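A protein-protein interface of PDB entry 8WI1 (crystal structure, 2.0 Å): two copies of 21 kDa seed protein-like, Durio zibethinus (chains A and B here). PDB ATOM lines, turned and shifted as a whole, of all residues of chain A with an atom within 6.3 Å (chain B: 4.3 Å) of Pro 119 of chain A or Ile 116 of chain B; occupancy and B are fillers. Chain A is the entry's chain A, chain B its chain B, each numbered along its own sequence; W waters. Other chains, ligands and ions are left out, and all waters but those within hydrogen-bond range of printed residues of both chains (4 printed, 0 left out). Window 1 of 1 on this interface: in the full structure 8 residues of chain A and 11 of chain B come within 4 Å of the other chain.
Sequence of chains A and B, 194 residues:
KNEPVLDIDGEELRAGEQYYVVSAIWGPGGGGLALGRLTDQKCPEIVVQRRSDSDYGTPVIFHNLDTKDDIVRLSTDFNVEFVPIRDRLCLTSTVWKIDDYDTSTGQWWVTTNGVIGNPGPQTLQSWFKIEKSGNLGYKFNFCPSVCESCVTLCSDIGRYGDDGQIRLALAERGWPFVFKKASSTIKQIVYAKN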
ATOM      1  N   LEU A  65      -1.093   6.377 -27.219  1.00  0.00           N
ATOM      2  CA  LEU A  65      -2.485   6.862 -27.168  1.00  0.00           C
ATOM      3  C   LEU A  65      -3.289   5.831 -27.944  1.00  0.00           C
ATOM      4  O   LEU A  65      -4.354   5.454 -27.477  1.00  0.00           O
ATOM      5  CB  LEU A  65      -2.551   8.224 -27.851  1.00  0.00           C
ATOM      6  CG  LEU A  65      -3.946   8.768 -28.132  1.00  0.00           C
ATOM      7  CD1 LEU A  65      -4.684   9.005 -26.834  1.00  0.00           C
ATOM      8  CD2 LEU A  65      -3.871  10.049 -28.940  1.00  0.00           C
ATOM      9  N   ASP A  66      -2.743   5.382 -29.071  1.00  0.00           N
ATOM     10  CA  ASP A  66      -3.418   4.381 -29.935  1.00  0.00           C
ATOM     11  C   ASP A  66      -2.849   2.997 -29.615  1.00  0.00           C
ATOM     12  O   ASP A  66      -1.736   2.705 -30.062  1.00  0.00           O
ATOM     13  CB  ASP A  66      -3.294   4.757 -31.410  1.00  0.00           C
ATOM     14  CG  ASP A  66      -4.006   3.815 -32.362  1.00  0.00           C
ATOM     15  OD1 ASP A  66      -4.671   2.886 -31.883  1.00  0.00           O
ATOM     16  OD2 ASP A  66      -3.893   4.027 -33.576  1.00  0.00           O
ATOM     17  N   LYS A  68      -3.531   0.285 -30.858  1.00  0.00           N
ATOM     18  CA  LYS A  68      -3.397  -0.534 -32.088  1.00  0.00           C
ATOM     19  C   LYS A  68      -2.005  -0.345 -32.702  1.00  0.00           C
ATOM     20  O   LYS A  68      -1.594  -1.213 -33.469  1.00  0.00           O
ATOM     21  CB  LYS A  68      -4.475  -0.155 -33.099  1.00  0.00           C
ATOM     22  CG  LYS A  68      -5.914  -0.261 -32.624  1.00  0.00           C
ATOM     23  CD  LYS A  68      -6.894  -0.131 -33.763  1.00  0.00           C
ATOM     24  CE  LYS A  68      -6.719   1.148 -34.552  1.00  0.00           C
ATOM     25  NZ  LYS A  68      -6.852   2.347 -33.694  1.00  0.00           N
ATOM     26  N   GLY A 117      -3.792   5.696 -20.185  1.00  0.00           N
ATOM     27  CA  GLY A 117      -5.005   5.636 -20.972  1.00  0.00           C
ATOM     28  C   GLY A 117      -6.041   6.668 -20.533  1.00  0.00           C
ATOM     29  O   GLY A 117      -5.726   7.704 -19.936  1.00  0.00           O
ATOM     30  N   ASN A 118      -7.301   6.360 -20.844  1.00  0.00           N
ATOM     31  CA  ASN A 118      -8.421   7.275 -20.649  1.00  0.00           C
ATOM     32  C   ASN A 118      -8.122   8.663 -21.233  1.00  0.00           C
ATOM     33  O   ASN A 118      -8.230   9.672 -20.531  1.00  0.00           O
ATOM     34  CB  ASN A 118      -8.786   7.384 -19.172  1.00  0.00           C
ATOM     35  CG  ASN A 118      -9.998   8.287 -18.922  1.00  0.00           C
ATOM     36  OD1 ASN A 118     -10.751   8.589 -19.842  1.00  0.00           O
ATOM     37  ND2 ASN A 118     -10.180   8.723 -17.677  1.00  0.00           N
ATOM     38  N   PRO A 119      -7.750   8.747 -22.512  1.00  0.00           N
ATOM     39  CA  PRO A 119      -7.419  10.061 -23.079  1.00  0.00           C
ATOM     40  C   PRO A 119      -8.605  11.009 -23.003  1.00  0.00           C
ATOM     41  O   PRO A 119      -9.736  10.652 -23.339  1.00  0.00           O
ATOM     42  CB  PRO A 119      -7.060   9.743 -24.538  1.00  0.00           C
ATOM     43  CG  PRO A 119      -7.775   8.455 -24.819  1.00  0.00           C
ATOM     44  CD  PRO A 119      -7.699   7.688 -23.539  1.00  0.00           C
ATOM     45  N   GLY A 120      -8.331  12.235 -22.585  1.00  0.00           N
ATOM     46  CA  GLY A 120      -9.363  13.236 -22.484  1.00  0.00           C
ATOM     47  C   GLY A 120      -9.023  14.206 -21.385  1.00  0.00           C
ATOM     48  O   GLY A 120      -7.881  14.261 -20.909  1.00  0.00           O
ATOM     49  N   PRO A 121     -10.019  14.980 -20.939  1.00  0.00           N
ATOM     50  CA  PRO A 121      -9.740  16.015 -19.933  1.00  0.00           C
ATOM     51  C   PRO A 121      -9.286  15.461 -18.599  1.00  0.00           C
ATOM     52  O   PRO A 121      -8.544  16.148 -17.882  1.00  0.00           O
ATOM     53  CB  PRO A 121     -11.081  16.765 -19.803  1.00  0.00           C
ATOM     54  CG  PRO A 121     -12.109  15.867 -20.407  1.00  0.00           C
ATOM     55  CD  PRO A 121     -11.396  15.061 -21.460  1.00  0.00           C
ATOM     56  N   GLN A 122      -9.704  14.251 -18.222  1.00  0.00           N
ATOM     57  CA  GLN A 122      -9.375  13.778 -16.878  1.00  0.00           C
ATOM     58  C   GLN A 122      -7.912  13.392 -16.759  1.00  0.00           C
ATOM     59  O   GLN A 122      -7.348  13.460 -15.659  1.00  0.00           O
ATOM     60  CB  GLN A 122     -10.252  12.595 -16.473  1.00  0.00           C
ATOM     61  CG  GLN A 122     -11.721  12.931 -16.388  1.00  0.00           C
ATOM     62  CD  GLN A 122     -12.481  12.359 -17.538  1.00  0.00           C
ATOM     63  OE1 GLN A 122     -12.094  11.329 -18.089  1.00  0.00           O
ATOM     64  NE2 GLN A 122     -13.574  13.006 -17.914  1.00  0.00           N
ATOM     65  N   THR A 123      -7.277  13.020 -17.878  1.00  0.00           N
ATOM     66  CA  THR A 123      -5.900  12.541 -17.881  1.00  0.00           C
ATOM     67  C   THR A 123      -4.935  13.497 -18.578  1.00  0.00           C
ATOM     68  O   THR A 123      -3.779  13.121 -18.811  1.00  0.00           O
ATOM     69  CB  THR A 123      -5.831  11.162 -18.545  1.00  0.00           C
ATOM     70  OG1 THR A 123      -6.388  11.252 -19.860  1.00  0.00           O
ATOM     71  CG2 THR A 123      -6.602  10.112 -17.736  1.00  0.00           C
ATOM     72  N   TRP A 127      -0.201  13.010 -20.474  1.00  0.00           N
ATOM     73  CA  TRP A 127       0.169  12.782 -21.866  1.00  0.00           C
ATOM     74  C   TRP A 127       1.410  13.587 -22.223  1.00  0.00           C
ATOM     75  O   TRP A 127       1.459  14.798 -21.982  1.00  0.00           O
ATOM     76  CB  TRP A 127      -0.987  13.133 -22.794  1.00  0.00           C
ATOM     77  CG  TRP A 127      -2.130  12.247 -22.539  1.00  0.00           C
ATOM     78  CD1 TRP A 127      -3.249  12.529 -21.804  1.00  0.00           C
ATOM     79  CD2 TRP A 127      -2.268  10.901 -22.991  1.00  0.00           C
ATOM     80  NE1 TRP A 127      -4.088  11.444 -21.786  1.00  0.00           N
ATOM     81  CE2 TRP A 127      -3.500  10.419 -22.488  1.00  0.00           C
ATOM     82  CE3 TRP A 127      -1.459  10.046 -23.745  1.00  0.00           C
ATOM     83  CZ2 TRP A 127      -3.951   9.126 -22.733  1.00  0.00           C
ATOM     84  CZ3 TRP A 127      -1.905   8.754 -23.997  1.00  0.00           C
ATOM     85  CH2 TRP A 127      -3.147   8.309 -23.495  1.00  0.00           C
ATOM     86  N   VAL A 146      -5.111  15.380 -26.525  1.00  0.00           N
ATOM     87  CA  VAL A 146      -6.204  14.443 -26.256  1.00  0.00           C
ATOM     88  C   VAL A 146      -7.539  15.122 -25.981  1.00  0.00           C
ATOM     89  O   VAL A 146      -8.584  14.454 -25.999  1.00  0.00           O
ATOM     90  CB  VAL A 146      -5.871  13.526 -25.060  1.00  0.00           C
ATOM     91  CG1 VAL A 146      -4.691  12.603 -25.396  1.00  0.00           C
ATOM     92  CG2 VAL A 146      -5.577  14.362 -23.792  1.00  0.00           C
ATOM     93  N   CYS A 147      -7.535  16.427 -25.715  1.00  0.00           N
ATOM     94  CA  CYS A 147      -8.728  17.165 -25.302  1.00  0.00           C
ATOM     95  C   CYS A 147      -8.751  18.438 -26.128  1.00  0.00           C
ATOM     96  O   CYS A 147      -8.151  19.437 -25.735  1.00  0.00           O
ATOM     97  CB  CYS A 147      -8.728  17.480 -23.817  1.00  0.00           C
ATOM     98  SG  CYS A 147     -10.135  18.526 -23.387  1.00  0.00           S
ATOM     99  N   HIS B  63     -11.014  -1.254 -23.748  1.00  0.00           N
ATOM    100  CA  HIS B  63     -10.398  -0.182 -22.974  1.00  0.00           C
ATOM    101  C   HIS B  63     -11.240   0.021 -21.724  1.00  0.00           C
ATOM    102  O   HIS B  63     -12.420   0.370 -21.829  1.00  0.00           O
ATOM    103  CB  HIS B  63     -10.307   1.126 -23.784  1.00  0.00           C
ATOM    104  CG  HIS B  63      -9.560   0.998 -25.080  1.00  0.00           C
ATOM    105  ND1 HIS B  63      -8.209   1.257 -25.191  1.00  0.00           N
ATOM    106  CD2 HIS B  63      -9.978   0.659 -26.322  1.00  0.00           C
ATOM    107  CE1 HIS B  63      -7.826   1.074 -26.443  1.00  0.00           C
ATOM    108  NE2 HIS B  63      -8.880   0.716 -27.153  1.00  0.00           N
ATOM    109  N   ASN B  79     -14.843   0.894 -23.495  1.00  0.00           N
ATOM    110  CA  ASN B  79     -14.769   1.159 -24.931  1.00  0.00           C
ATOM    111  C   ASN B  79     -14.288  -0.096 -25.658  1.00  0.00           C
ATOM    112  O   ASN B  79     -13.440  -0.830 -25.139  1.00  0.00           O
ATOM    113  CB  ASN B  79     -13.791   2.295 -25.278  1.00  0.00           C
ATOM    114  CG  ASN B  79     -14.079   3.596 -24.554  1.00  0.00           C
ATOM    115  OD1 ASN B  79     -13.165   4.210 -23.983  1.00  0.00           O
ATOM    116  ND2 ASN B  79     -15.336   4.037 -24.588  1.00  0.00           N
ATOM    117  N   GLU B  81     -12.921  -1.372 -29.694  1.00  0.00           N
ATOM    118  CA  GLU B  81     -12.338  -0.834 -30.912  1.00  0.00           C
ATOM    119  C   GLU B  81     -11.846  -1.986 -31.775  1.00  0.00           C
ATOM    120  O   GLU B  81     -11.187  -2.893 -31.268  1.00  0.00           O
ATOM    121  CB  GLU B  81     -11.207   0.128 -30.531  1.00  0.00           C
ATOM    122  CG  GLU B  81     -10.052   0.176 -31.438  1.00  0.00           C
ATOM    123  CD  GLU B  81      -9.036   1.214 -31.006  1.00  0.00           C
ATOM    124  OE1 GLU B  81      -8.512   1.125 -29.870  1.00  0.00           O
ATOM    125  OE2 GLU B  81      -8.776   2.126 -31.811  1.00  0.00           O
ATOM    126  N   VAL B  95     -13.644   2.644 -33.321  1.00  0.00           N
ATOM    127  CA  VAL B  95     -14.276   2.490 -32.008  1.00  0.00           C
ATOM    128  C   VAL B  95     -15.784   2.355 -32.178  1.00  0.00           C
ATOM    129  O   VAL B  95     -16.418   3.175 -32.852  1.00  0.00           O
ATOM    130  CB  VAL B  95     -13.933   3.685 -31.103  1.00  0.00           C
ATOM    131  CG1 VAL B  95     -14.634   3.556 -29.720  1.00  0.00           C
ATOM    132  CG2 VAL B  95     -12.409   3.829 -30.983  1.00  0.00           C
ATOM    133  N   VAL B 115     -15.476   7.116 -29.686  1.00  0.00           N
ATOM    134  CA  VAL B 115     -14.390   7.810 -29.003  1.00  0.00           C
ATOM    135  C   VAL B 115     -13.928   6.960 -27.834  1.00  0.00           C
ATOM    136  O   VAL B 115     -14.753   6.466 -27.060  1.00  0.00           O
ATOM    137  CB  VAL B 115     -14.826   9.209 -28.519  1.00  0.00           C
ATOM    138  CG1 VAL B 115     -13.717   9.850 -27.704  1.00  0.00           C
ATOM    139  CG2 VAL B 115     -15.171  10.081 -29.702  1.00  0.00           C
ATOM    140  N   ILE B 116     -12.612   6.785 -27.710  1.00  0.00           N
ATOM    141  CA  ILE B 116     -12.029   6.155 -26.533  1.00  0.00           C
ATOM    142  C   ILE B 116     -11.872   7.212 -25.455  1.00  0.00           C
ATOM    143  O   ILE B 116     -11.304   8.281 -25.697  1.00  0.00           O
ATOM    144  CB  ILE B 116     -10.667   5.526 -26.871  1.00  0.00           C
ATOM    145  CG1 ILE B 116     -10.845   4.313 -27.785  1.00  0.00           C
ATOM    146  CG2 ILE B 116      -9.901   5.162 -25.597  1.00  0.00           C
ATOM    147  CD1 ILE B 116      -9.674   4.095 -28.703  1.00  0.00           C
ATOM    148  N   GLY B 117     -12.386   6.936 -24.270  1.00  0.00           N
ATOM    149  CA  GLY B 117     -12.027   7.730 -23.112  1.00  0.00           C
ATOM    150  C   GLY B 117     -13.030   8.831 -22.811  1.00  0.00           C
ATOM    151  O   GLY B 117     -14.088   8.959 -23.436  1.00  0.00           O
ATOM    152  N   ASN B 118     -12.666   9.634 -21.813  1.00  0.00           N
ATOM    153  CA  ASN B 118     -13.474  10.757 -21.350  1.00  0.00           C
ATOM    154  C   ASN B 118     -14.898  10.323 -20.986  1.00  0.00           C
ATOM    155  O   ASN B 118     -15.868  10.802 -21.583  1.00  0.00           O
ATOM    156  CB  ASN B 118     -13.500  11.866 -22.393  1.00  0.00           C
ATOM    157  CG  ASN B 118     -14.180  13.138 -21.879  1.00  0.00           C
ATOM    158  OD1 ASN B 118     -14.282  13.361 -20.665  1.00  0.00           O
ATOM    159  ND2 ASN B 118     -14.633  13.975 -22.797  1.00  0.00           N
HETATM  160  O   HOH W   1      -7.052   4.997 -31.086  1.00  0.00           O
HETATM  161  O   HOH W   2      -6.754   2.891 -29.482  1.00  0.00           O
HETATM  162  O   HOH W   3     -11.432  11.002 -25.118  1.00  0.00           O
HETATM  163  O   HOH W   4      -9.839   3.828 -33.968  1.00  0.00           O
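Asn 118 of chain A touches Gly 117 of chain B, but with the chains exchanged Gly 117 of chain A does not touch Asn 118 of chain B (7.4 Å).
Asn 118 of chain B touches its own counterpart, Asn 118 of chain A.
Of the 8 pairs that touch across the chains among the printed residues, 1 has its exchanged pair printed and touching as well.
The side-chain carboxylate (OD1) of Asp 66 of chain A lies within salt-bridge range of the side-chain amino group (NZ) of Lys 68 of chain A (2.9 Å).
OE1 of Gln 122 of chain A is in hydrogen-bond range of ND2 of Asn 118 of chain A (3.3 Å).
The side-chain hydroxyl (OG1) of Thr 123 of chain A is in hydrogen-bond range of the backbone carbonyl oxygen (O) of Asn 118 of chain A (2.5 Å).
NE2 of His 63 of chain B lies within hydrogen-bond range of OE1 of Glu 81 of chain B (2.8 Å).
OD1 of Asn 79 of chain B lies within hydrogen-bond range of N of Gly 117 of chain B (2.8 Å).
Pro 119 of chain A touches three residues of chain B.
Ile 116 of chain B touches just one residue of chain A: Pro 119.
Of the printed residues of chain A, Gly 117 of chain B touches Asn 118 and Pro 119.
Printed residues of chain B within 4 Å of Pro 121 of chain A: Asn 118 (3.3 Å).
Of the printed residues of chain A, Asn 118 of chain B touches Asn 118 (2.9 Å), Pro 119 (3.5 Å), Pro 121 (3.3 Å) and Gln 122 (2.9 Å).
The nearest residue of chain A that does not touch Ile 116 of chain B is Asn 118 of chain A (5.5 Å).
The nearest printed residue of chain B that does not touch Pro 121 of chain A is Gly 117 of chain B (6.6 Å).
Of the 8 printed residues of chain B, 4 touch a printed residue of chain A.
Hydrophobic or aromatic side chains of chain B within 4 Å of the printed part of chain A: Ile 116.
Of the 13 printed residues of chain A, 5 touch a printed residue of chain B.
Printed residues of chain A that touch a printed residue of chain B: Lys 68, Asn 118, Pro 119, Pro 121 and Gln 122.
Hydrophobic or aromatic side chains of chain A that line the printed part of chain B: Pro 119 and Pro 121.
Water W3 bridges O of Pro 119 of chain A (2.5 Å) and O of Ile 116 of chain B (2.8 Å).
Water W2 lies within hydrogen-bond range of the side-chain carboxylate of Glu 81 of chain B (2.5 Å) and the side-chain carboxylate of Asp 66 of chain A (3.2 Å).
Water W4 bridges OE2 of Glu 81 of chain B (2.9 Å) and NZ of Lys 68 of chain A (3.3 Å).
Water W1 lies within hydrogen-bond range of OD1 of Asp 66 of chain A (3.3 Å) and OE2 of Glu 81 of chain B (3.4 Å).
NZ of Lys 68 of chain A lies within salt-bridge range of OE2 of Glu 81 of chain B.
OD1 of Asn 118 of chain A lies within hydrogen-bond range of N of Asn 118 of chain B (2.9 Å).
O of Pro 119 of chain A lies within hydrogen-bond range of N of Asn 118 of chain B, 3.5 Å away.
NE2 of Gln 122 of chain A is in hydrogen-bond range of OD1 of Asn 118 of chain B, 2.9 Å away.
Among the printed residues, merely in contact across the chains: Asn 118 of chain A with Gly 117 of chain B (3.6 Å), Pro 119 of chain A with Ile 116 of chain B (3.6 Å), Pro 119 of chain A with Gly 117 of chain B (3.7 Å) and Pro 121 of chain A with Asn 118 of chain B (3.3 Å).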
